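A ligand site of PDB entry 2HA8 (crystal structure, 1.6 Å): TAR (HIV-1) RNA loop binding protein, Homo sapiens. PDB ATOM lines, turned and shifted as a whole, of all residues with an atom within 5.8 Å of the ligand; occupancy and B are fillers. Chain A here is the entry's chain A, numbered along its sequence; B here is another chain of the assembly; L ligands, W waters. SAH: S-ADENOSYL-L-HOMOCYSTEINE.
Water W1 lies within hydrogen-bond range of the side-chain amide oxygen of Gln 108 (2.5 Å), the side-chain carboxylate of Glu 107 (2.7 Å) and a nitrogen (N) of the ligand (2.7 Å).
Water W2 lies within hydrogen-bond range of N of the ligand (3.0 Å), O of Gln 108 (3.0 Å) and OE2 of Glu 107 (3.5 Å).
Water W3 lies within hydrogen-bond range of NH2 of Arg 45 of chain B (2.9 Å), O of Leu 158 (3.0 Å), SD of the ligand (3.3 Å) and OG of Ser 157 (3.5 Å).
O of Val 147 sits at hydrogen-bond distance from N of Glu 107 (3.0 Å).
NE2 of Gln 151 lies close to NE2 of Gln 108.
The side-chain amide oxygen (OE1) of Gln 151 lies close to the backbone carbonyl oxygen (O) of Arg 156 (3.2 Å).
NH2 of Arg 45 of chain B is in hydrogen-bond range of O of Leu 158, 3.4 Å away.
The side-chain amide nitrogen (NE2) of Gln 108 lies within hydrogen-bond range of the backbone carbonyl oxygen (O) of Arg 156 (3.2 Å).
The backbone NH (N) of Arg 132 is in hydrogen-bond range of the side-chain amide oxygen (OD1) of Asn 130, 2.9 Å away.
The side-chain amide oxygen (OD1) of Asn 130 sits at hydrogen-bond distance from the backbone NH (N) of Glu 133.
The backbone carbonyl oxygen (O) of Ser 157 lies within hydrogen-bond range of the guanidinium group (NE) of Arg 45 of chain B (3.0 Å).
Leu 128 touches the ligand.
Asn 130 touches the ligand (O to C5', 3.5 Å).
O of Glu 131 touches CG of the ligand, at 3.4 Å.
Arg 132 touches the ligand (O to CB, 3.9 Å).
CA of Gly 134 touches O3' of the ligand, at 3.3 Å.
O of Val 147 touches C2 of the ligand (3.9 Å).
Glu 148 touches the ligand.
Ser 157 touches the ligand.
CA of Val 160 touches O4' of the ligand, 3.5 Å away.
Hydrophobic or aromatic side chains within 4 Å of the ligand: Val 106, Ile 149, Leu 158 and Val 160.
Of the 25 residues printed, 18 come within 4 Å of the ligand.
Along chain A the residues within 4 Å of the ligand span positions 106 to 163.
The nearest printed residue that does not touch the ligand is Ile 135 (4.2 Å).
The backbone carbonyl oxygen (O) of Val 106 is in hydrogen-bond range of an oxygen (O2') of the ligand.
N of the ligand lies within salt-bridge range of OE2 of Glu 107 (3.9 Å).
A nitrogen (N6) of the ligand sits close to the side-chain amide nitrogen of Gln 151 (2.8 Å).
A nitrogen (N1) of the ligand lies within hydrogen-bond range of the backbone NH of Ile 149 (2.9 Å).
The backbone carbonyl oxygen (O) of Ile 149 sits at hydrogen-bond distance from a nitrogen (N6) of the ligand.
The backbone NH (N) of Gly 129 is in hydrogen-bond range of an oxygen (O2') of the ligand.
N of Leu 158 is in hydrogen-bond range of N7 of the ligand, 3.0 Å away.
OG of Ser 163 lies close to N7 of the ligand (3.5 Å).
A nitrogen (N6) of the ligand lies close to the side-chain amide nitrogen (NE2) of Gln 108, at 3.4 Å.
An oxygen (OXT) of the ligand is in salt-bridge range of the guanidinium group (NE) of Arg 156 (3.4 Å).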
ATOM      1  N   VAL A 106     -12.504  -7.970  24.826  1.00  0.00           N
ATOM      2  CA  VAL A 106     -13.699  -8.779  24.921  1.00  0.00           C
ATOM      3  C   VAL A 106     -13.228 -10.183  25.289  1.00  0.00           C
ATOM      4  O   VAL A 106     -12.687 -10.923  24.448  1.00  0.00           O
ATOM      5  CB  VAL A 106     -14.470  -8.789  23.592  1.00  0.00           C
ATOM      6  CG1 VAL A 106     -15.741  -9.662  23.701  1.00  0.00           C
ATOM      7  CG2 VAL A 106     -14.806  -7.347  23.162  1.00  0.00           C
ATOM      8  N   GLU A 107     -13.373 -10.529  26.559  1.00  0.00           N
ATOM      9  CA  GLU A 107     -12.750 -11.767  27.030  1.00  0.00           C
ATOM     10  C   GLU A 107     -13.208 -12.148  28.422  1.00  0.00           C
ATOM     11  O   GLU A 107     -13.507 -11.295  29.256  1.00  0.00           O
ATOM     12  CB  GLU A 107     -11.228 -11.623  27.000  1.00  0.00           C
ATOM     13  CG  GLU A 107     -10.434 -12.930  27.287  1.00  0.00           C
ATOM     14  CD  GLU A 107     -10.804 -14.073  26.355  1.00  0.00           C
ATOM     15  OE1 GLU A 107     -10.001 -14.341  25.438  1.00  0.00           O
ATOM     16  OE2 GLU A 107     -11.907 -14.681  26.493  1.00  0.00           O
ATOM     17  N   GLN A 108     -13.215 -13.458  28.660  1.00  0.00           N
ATOM     18  CA  GLN A 108     -13.566 -14.030  29.963  1.00  0.00           C
ATOM     19  C   GLN A 108     -12.269 -14.067  30.784  1.00  0.00           C
ATOM     20  O   GLN A 108     -11.332 -14.791  30.413  1.00  0.00           O
ATOM     21  CB  GLN A 108     -14.140 -15.443  29.794  1.00  0.00           C
ATOM     22  CG  GLN A 108     -15.393 -15.503  28.914  1.00  0.00           C
ATOM     23  CD  GLN A 108     -15.803 -16.927  28.587  1.00  0.00           C
ATOM     24  OE1 GLN A 108     -15.174 -17.607  27.775  1.00  0.00           O
ATOM     25  NE2 GLN A 108     -16.858 -17.376  29.230  1.00  0.00           N
ATOM     26  N   LEU A 127     -11.612  -5.203  21.280  1.00  0.00           N
ATOM     27  CA  LEU A 127     -10.556  -6.123  20.836  1.00  0.00           C
ATOM     28  C   LEU A 127     -11.029  -7.546  21.081  1.00  0.00           C
ATOM     29  O   LEU A 127     -11.205  -7.958  22.233  1.00  0.00           O
ATOM     30  CB  LEU A 127      -9.239  -5.854  21.596  1.00  0.00           C
ATOM     31  CG  LEU A 127      -8.072  -6.776  21.218  1.00  0.00           C
ATOM     32  CD1 LEU A 127      -7.640  -6.605  19.750  1.00  0.00           C
ATOM     33  CD2 LEU A 127      -6.860  -6.523  22.131  1.00  0.00           C
ATOM     34  N   LEU A 128     -11.289  -8.273  19.993  1.00  0.00           N
ATOM     35  CA  LEU A 128     -11.723  -9.674  20.089  1.00  0.00           C
ATOM     36  C   LEU A 128     -10.526 -10.630  20.110  1.00  0.00           C
ATOM     37  O   LEU A 128      -9.470 -10.331  19.552  1.00  0.00           O
ATOM     38  CB  LEU A 128     -12.652 -10.014  18.918  1.00  0.00           C
ATOM     39  CG  LEU A 128     -13.984  -9.260  18.930  1.00  0.00           C
ATOM     40  CD1 LEU A 128     -14.564  -9.247  17.513  1.00  0.00           C
ATOM     41  CD2 LEU A 128     -14.933  -9.909  19.916  1.00  0.00           C
ATOM     42  N   GLY A 129     -10.698 -11.779  20.762  1.00  0.00           N
ATOM     43  CA  GLY A 129      -9.587 -12.728  20.873  1.00  0.00           C
ATOM     44  C   GLY A 129      -9.519 -13.719  19.726  1.00  0.00           C
ATOM     45  O   GLY A 129     -10.473 -13.916  18.966  1.00  0.00           O
ATOM     46  N   ASN A 130      -8.371 -14.374  19.620  1.00  0.00           N
ATOM     47  CA  ASN A 130      -8.202 -15.501  18.694  1.00  0.00           C
ATOM     48  C   ASN A 130      -9.106 -16.678  19.066  1.00  0.00           C
ATOM     49  O   ASN A 130      -9.393 -16.900  20.243  1.00  0.00           O
ATOM     50  CB  ASN A 130      -6.745 -15.925  18.757  1.00  0.00           C
ATOM     51  CG  ASN A 130      -6.456 -17.091  17.878  1.00  0.00           C
ATOM     52  OD1 ASN A 130      -6.328 -18.223  18.360  1.00  0.00           O
ATOM     53  ND2 ASN A 130      -6.365 -16.853  16.575  1.00  0.00           N
ATOM     54  N   GLU A 131      -9.572 -17.443  18.074  1.00  0.00           N
ATOM     55  CA  GLU A 131     -10.508 -18.545  18.336  1.00  0.00           C
ATOM     56  C   GLU A 131      -9.921 -19.567  19.306  1.00  0.00           C
ATOM     57  O   GLU A 131     -10.644 -20.156  20.105  1.00  0.00           O
ATOM     58  CB  GLU A 131     -10.891 -19.258  17.031  1.00  0.00           C
ATOM     59  CG  GLU A 131     -11.716 -18.416  16.040  1.00  0.00           C
ATOM     60  CD  GLU A 131     -10.884 -17.630  15.038  1.00  0.00           C
ATOM     61  OE1 GLU A 131      -9.712 -17.280  15.323  1.00  0.00           O
ATOM     62  OE2 GLU A 131     -11.422 -17.363  13.944  1.00  0.00           O
ATOM     63  N   ARG A 132      -8.625 -19.807  19.201  1.00  0.00           N
ATOM     64  CA  ARG A 132      -7.957 -20.836  20.005  1.00  0.00           C
ATOM     65  C   ARG A 132      -7.324 -20.212  21.241  1.00  0.00           C
ATOM     66  O   ARG A 132      -7.466 -20.728  22.356  1.00  0.00           O
ATOM     67  CB  ARG A 132      -6.881 -21.536  19.170  1.00  0.00           C
ATOM     68  CG  ARG A 132      -7.394 -22.681  18.319  1.00  0.00           C
ATOM     69  CD  ARG A 132      -6.243 -23.442  17.615  1.00  0.00           C
ATOM     70  NE  ARG A 132      -6.020 -22.959  16.242  1.00  0.00           N
ATOM     71  CZ  ARG A 132      -5.032 -23.358  15.449  1.00  0.00           C
ATOM     72  NH1 ARG A 132      -4.129 -24.239  15.870  1.00  0.00           N
ATOM     73  NH2 ARG A 132      -4.918 -22.866  14.214  1.00  0.00           N
ATOM     74  N   GLU A 133      -6.636 -19.088  21.050  1.00  0.00           N
ATOM     75  CA  GLU A 133      -5.737 -18.533  22.048  1.00  0.00           C
ATOM     76  C   GLU A 133      -6.340 -17.384  22.863  1.00  0.00           C
ATOM     77  O   GLU A 133      -5.752 -16.977  23.860  1.00  0.00           O
ATOM     78  CB  GLU A 133      -4.456 -18.030  21.381  1.00  0.00           C
ATOM     79  CG  GLU A 133      -3.901 -18.895  20.228  1.00  0.00           C
ATOM     80  CD  GLU A 133      -3.186 -20.151  20.695  1.00  0.00           C
ATOM     81  OE1 GLU A 133      -3.502 -20.679  21.792  1.00  0.00           O
ATOM     82  OE2 GLU A 133      -2.295 -20.627  19.945  1.00  0.00           O
ATOM     83  N   GLY A 134      -7.498 -16.860  22.457  1.00  0.00           N
ATOM     84  CA  GLY A 134      -8.048 -15.674  23.144  1.00  0.00           C
ATOM     85  C   GLY A 134      -7.164 -14.439  22.918  1.00  0.00           C
ATOM     86  O   GLY A 134      -6.498 -14.323  21.897  1.00  0.00           O
ATOM     87  N   ILE A 135      -7.148 -13.523  23.886  1.00  0.00           N
ATOM     88  CA  ILE A 135      -6.289 -12.350  23.796  1.00  0.00           C
ATOM     89  C   ILE A 135      -4.916 -12.677  24.426  1.00  0.00           C
ATOM     90  O   ILE A 135      -4.873 -13.119  25.571  1.00  0.00           O
ATOM     91  CB  ILE A 135      -6.942 -11.118  24.492  1.00  0.00           C
ATOM     92  CG1 ILE A 135      -8.312 -10.781  23.862  1.00  0.00           C
ATOM     93  CG2 ILE A 135      -6.016  -9.898  24.402  1.00  0.00           C
ATOM     94  CD1 ILE A 135      -9.037  -9.628  24.539  1.00  0.00           C
ATOM     95  N   VAL A 147     -14.242  -6.876  29.182  1.00  0.00           N
ATOM     96  CA  VAL A 147     -15.682  -7.085  29.351  1.00  0.00           C
ATOM     97  C   VAL A 147     -16.030  -8.516  28.956  1.00  0.00           C
ATOM     98  O   VAL A 147     -15.550  -9.006  27.941  1.00  0.00           O
ATOM     99  CB  VAL A 147     -16.526  -6.033  28.571  1.00  0.00           C
ATOM    100  CG1 VAL A 147     -18.027  -6.361  28.602  1.00  0.00           C
ATOM    101  CG2 VAL A 147     -16.283  -4.648  29.164  1.00  0.00           C
ATOM    102  N   GLU A 148     -16.835  -9.167  29.790  1.00  0.00           N
ATOM    103  CA  GLU A 148     -17.259 -10.529  29.524  1.00  0.00           C
ATOM    104  C   GLU A 148     -18.773 -10.646  29.475  1.00  0.00           C
ATOM    105  O   GLU A 148     -19.518  -9.941  30.205  1.00  0.00           O
ATOM    106  CB  GLU A 148     -16.624 -11.528  30.502  1.00  0.00           C
ATOM    107  CG  GLU A 148     -17.141 -11.457  31.908  1.00  0.00           C
ATOM    108  CD  GLU A 148     -16.512 -12.509  32.846  1.00  0.00           C
ATOM    109  OE1 GLU A 148     -15.475 -13.123  32.509  1.00  0.00           O
ATOM    110  OE2 GLU A 148     -17.083 -12.719  33.944  1.00  0.00           O
ATOM    111  N   ILE A 149     -19.234 -11.531  28.601  1.00  0.00           N
ATOM    112  CA  ILE A 149     -20.648 -11.868  28.500  1.00  0.00           C
ATOM    113  C   ILE A 149     -20.921 -12.984  29.495  1.00  0.00           C
ATOM    114  O   ILE A 149     -20.268 -14.013  29.413  1.00  0.00           O
ATOM    115  CB  ILE A 149     -20.947 -12.380  27.083  1.00  0.00           C
ATOM    116  CG1 ILE A 149     -20.588 -11.302  26.043  1.00  0.00           C
ATOM    117  CG2 ILE A 149     -22.401 -12.777  26.956  1.00  0.00           C
ATOM    118  CD1 ILE A 149     -20.278 -11.850  24.650  1.00  0.00           C
ATOM    119  N   PRO A 150     -21.870 -12.784  30.432  1.00  0.00           N
ATOM    120  CA  PRO A 150     -22.138 -13.870  31.418  1.00  0.00           C
ATOM    121  C   PRO A 150     -22.772 -15.098  30.752  1.00  0.00           C
ATOM    122  O   PRO A 150     -23.608 -14.947  29.860  1.00  0.00           O
ATOM    123  CB  PRO A 150     -23.127 -13.225  32.392  1.00  0.00           C
ATOM    124  CG  PRO A 150     -23.805 -12.148  31.587  1.00  0.00           C
ATOM    125  CD  PRO A 150     -22.732 -11.617  30.644  1.00  0.00           C
ATOM    126  N   GLN A 151     -22.376 -16.294  31.187  1.00  0.00           N
ATOM    127  CA  GLN A 151     -22.883 -17.541  30.609  1.00  0.00           C
ATOM    128  C   GLN A 151     -23.581 -18.384  31.681  1.00  0.00           C
ATOM    129  O   GLN A 151     -23.306 -18.216  32.877  1.00  0.00           O
ATOM    130  CB  GLN A 151     -21.737 -18.342  29.978  1.00  0.00           C
ATOM    131  CG  GLN A 151     -21.003 -17.615  28.863  1.00  0.00           C
ATOM    132  CD  GLN A 151     -20.002 -18.475  28.146  1.00  0.00           C
ATOM    133  OE1 GLN A 151     -19.816 -19.670  28.462  1.00  0.00           O
ATOM    134  NE2 GLN A 151     -19.360 -17.911  27.162  1.00  0.00           N
ATOM    135  N   ARG A 156     -17.919 -23.736  27.320  1.00  0.00           N
ATOM    136  CA  ARG A 156     -17.005 -22.772  27.956  1.00  0.00           C
ATOM    137  C   ARG A 156     -17.068 -21.354  27.421  1.00  0.00           C
ATOM    138  O   ARG A 156     -16.760 -20.408  28.147  1.00  0.00           O
ATOM    139  CB  ARG A 156     -15.554 -23.273  27.929  1.00  0.00           C
ATOM    140  CG  ARG A 156     -14.971 -23.579  26.548  1.00  0.00           C
ATOM    141  CD  ARG A 156     -13.705 -24.452  26.688  1.00  0.00           C
ATOM    142  NE  ARG A 156     -12.787 -23.905  27.694  1.00  0.00           N
ATOM    143  CZ  ARG A 156     -11.952 -24.627  28.433  1.00  0.00           C
ATOM    144  NH1 ARG A 156     -11.862 -25.948  28.270  1.00  0.00           N
ATOM    145  NH2 ARG A 156     -11.178 -24.031  29.334  1.00  0.00           N
ATOM    146  N   SER A 157     -17.419 -21.207  26.153  1.00  0.00           N
ATOM    147  CA  SER A 157     -17.329 -19.892  25.478  1.00  0.00           C
ATOM    148  C   SER A 157     -18.315 -19.792  24.329  1.00  0.00           C
ATOM    149  O   SER A 157     -18.778 -20.806  23.821  1.00  0.00           O
ATOM    150  CB  SER A 157     -15.912 -19.683  24.961  1.00  0.00           C
ATOM    151  OG  SER A 157     -15.595 -20.637  23.954  1.00  0.00           O
ATOM    152  N   LEU A 158     -18.606 -18.566  23.910  1.00  0.00           N
ATOM    153  CA  LEU A 158     -19.321 -18.314  22.677  1.00  0.00           C
ATOM    154  C   LEU A 158     -18.371 -18.305  21.484  1.00  0.00           C
ATOM    155  O   LEU A 158     -17.154 -18.185  21.652  1.00  0.00           O
ATOM    156  CB  LEU A 158     -20.026 -16.957  22.780  1.00  0.00           C
ATOM    157  CG  LEU A 158     -21.176 -16.874  23.794  1.00  0.00           C
ATOM    158  CD1 LEU A 158     -21.419 -15.405  24.152  1.00  0.00           C
ATOM    159  CD2 LEU A 158     -22.458 -17.491  23.185  1.00  0.00           C
ATOM    160  N   ASN A 159     -18.926 -18.427  20.285  1.00  0.00           N
ATOM    161  CA  ASN A 159     -18.177 -18.155  19.083  1.00  0.00           C
ATOM    162  C   ASN A 159     -17.721 -16.674  19.090  1.00  0.00           C
ATOM    163  O   ASN A 159     -18.434 -15.792  19.623  1.00  0.00           O
ATOM    164  CB  ASN A 159     -19.051 -18.445  17.855  1.00  0.00           C
ATOM    165  CG  ASN A 159     -18.487 -17.878  16.586  1.00  0.00           C
ATOM    166  OD1 ASN A 159     -18.809 -16.735  16.218  1.00  0.00           O
ATOM    167  ND2 ASN A 159     -17.685 -18.662  15.874  1.00  0.00           N
ATOM    168  N   VAL A 160     -16.541 -16.429  18.530  1.00  0.00           N
ATOM    169  CA  VAL A 160     -15.961 -15.064  18.623  1.00  0.00           C
ATOM    170  C   VAL A 160     -16.791 -13.995  17.864  1.00  0.00           C
ATOM    171  O   VAL A 160     -16.924 -12.865  18.351  1.00  0.00           O
ATOM    172  CB  VAL A 160     -14.475 -15.025  18.193  1.00  0.00           C
ATOM    173  CG1 VAL A 160     -14.324 -15.342  16.716  1.00  0.00           C
ATOM    174  CG2 VAL A 160     -13.823 -13.662  18.536  1.00  0.00           C
ATOM    175  N   SER A 163     -19.847 -13.292  19.921  1.00  0.00           N
ATOM    176  CA  SER A 163     -19.411 -12.455  21.059  1.00  0.00           C
ATOM    177  C   SER A 163     -19.316 -10.982  20.625  1.00  0.00           C
ATOM    178  O   SER A 163     -19.832 -10.094  21.290  1.00  0.00           O
ATOM    179  CB  SER A 163     -18.037 -12.917  21.574  1.00  0.00           C
ATOM    180  OG  SER A 163     -18.123 -14.238  22.094  1.00  0.00           O
ATOM    181  N   LEU A 167     -21.624  -7.499  21.823  1.00  0.00           N
ATOM    182  CA  LEU A 167     -21.101  -6.206  22.335  1.00  0.00           C
ATOM    183  C   LEU A 167     -21.439  -5.051  21.401  1.00  0.00           C
ATOM    184  O   LEU A 167     -21.728  -3.962  21.872  1.00  0.00           O
ATOM    185  CB  LEU A 167     -19.608  -6.257  22.617  1.00  0.00           C
ATOM    186  CG  LEU A 167     -19.323  -6.753  24.040  1.00  0.00           C
ATOM    187  CD1 LEU A 167     -19.487  -8.283  24.106  1.00  0.00           C
ATOM    188  CD2 LEU A 167     -17.993  -6.333  24.595  1.00  0.00           C
ATOM    189  N   ARG B  45     -25.048 -23.816  19.917  1.00  0.00           N
ATOM    190  CA  ARG B  45     -24.038 -23.396  20.896  1.00  0.00           C
ATOM    191  C   ARG B  45     -24.533 -22.164  21.689  1.00  0.00           C
ATOM    192  O   ARG B  45     -24.449 -22.132  22.907  1.00  0.00           O
ATOM    193  CB  ARG B  45     -22.727 -23.115  20.168  1.00  0.00           C
ATOM    194  CG  ARG B  45     -21.592 -22.610  21.083  1.00  0.00           C
ATOM    195  CD  ARG B  45     -20.396 -22.196  20.240  1.00  0.00           C
ATOM    196  NE  ARG B  45     -19.233 -21.956  21.082  1.00  0.00           N
ATOM    197  CZ  ARG B  45     -17.986 -21.847  20.621  1.00  0.00           C
ATOM    198  NH1 ARG B  45     -17.740 -21.928  19.307  1.00  0.00           N
ATOM    199  NH2 ARG B  45     -16.998 -21.618  21.473  1.00  0.00           N
HETATM  200  N   SAH L   1     -11.214 -18.446  25.916  1.00  0.00           N
HETATM  201  CA  SAH L   1     -11.728 -19.494  24.991  1.00  0.00           C
HETATM  202  CB  SAH L   1     -10.937 -19.473  23.694  1.00  0.00           C
HETATM  203  CG  SAH L   1     -11.261 -18.279  22.829  1.00  0.00           C
HETATM  204  SD  SAH L   1     -13.043 -18.011  22.665  1.00  0.00           S
HETATM  205  C   SAH L   1     -11.666 -20.888  25.616  1.00  0.00           C
HETATM  206  O   SAH L   1     -11.109 -21.042  26.706  1.00  0.00           O
HETATM  207  OXT SAH L   1     -12.169 -21.875  25.057  1.00  0.00           O
HETATM  208  C5' SAH L   1     -12.678 -16.824  21.344  1.00  0.00           C
HETATM  209  C4' SAH L   1     -13.006 -15.373  21.686  1.00  0.00           C
HETATM  210  O4' SAH L   1     -14.395 -15.193  21.742  1.00  0.00           O
HETATM  211  C3' SAH L   1     -12.468 -14.869  23.017  1.00  0.00           C
HETATM  212  O3' SAH L   1     -11.106 -14.523  23.003  1.00  0.00           O
HETATM  213  C2' SAH L   1     -13.365 -13.675  23.270  1.00  0.00           C
HETATM  214  O2' SAH L   1     -12.960 -12.533  22.497  1.00  0.00           O
HETATM  215  C1' SAH L   1     -14.679 -14.200  22.720  1.00  0.00           C
HETATM  216  N9  SAH L   1     -15.594 -14.786  23.726  1.00  0.00           N
HETATM  217  C8  SAH L   1     -16.164 -16.066  23.721  1.00  0.00           C
HETATM  218  N7  SAH L   1     -17.011 -16.135  24.764  1.00  0.00           N
HETATM  219  C5  SAH L   1     -17.010 -14.959  25.437  1.00  0.00           C
HETATM  220  C6  SAH L   1     -17.657 -14.470  26.569  1.00  0.00           C
HETATM  221  N6  SAH L   1     -18.524 -15.206  27.277  1.00  0.00           N
HETATM  222  N1  SAH L   1     -17.417 -13.166  26.960  1.00  0.00           N
HETATM  223  C2  SAH L   1     -16.562 -12.347  26.276  1.00  0.00           C
HETATM  224  N3  SAH L   1     -15.895 -12.823  25.173  1.00  0.00           N
HETATM  225  C4  SAH L   1     -16.126 -14.109  24.767  1.00  0.00           C
HETATM  226  O   HOH W   1     -13.463 -16.875  26.055  1.00  0.00           O
HETATM  227  O   HOH W   2     -11.089 -17.272  28.675  1.00  0.00           O
HETATM  228  O   HOH W   3     -14.870 -19.852  20.634  1.00  0.00           O
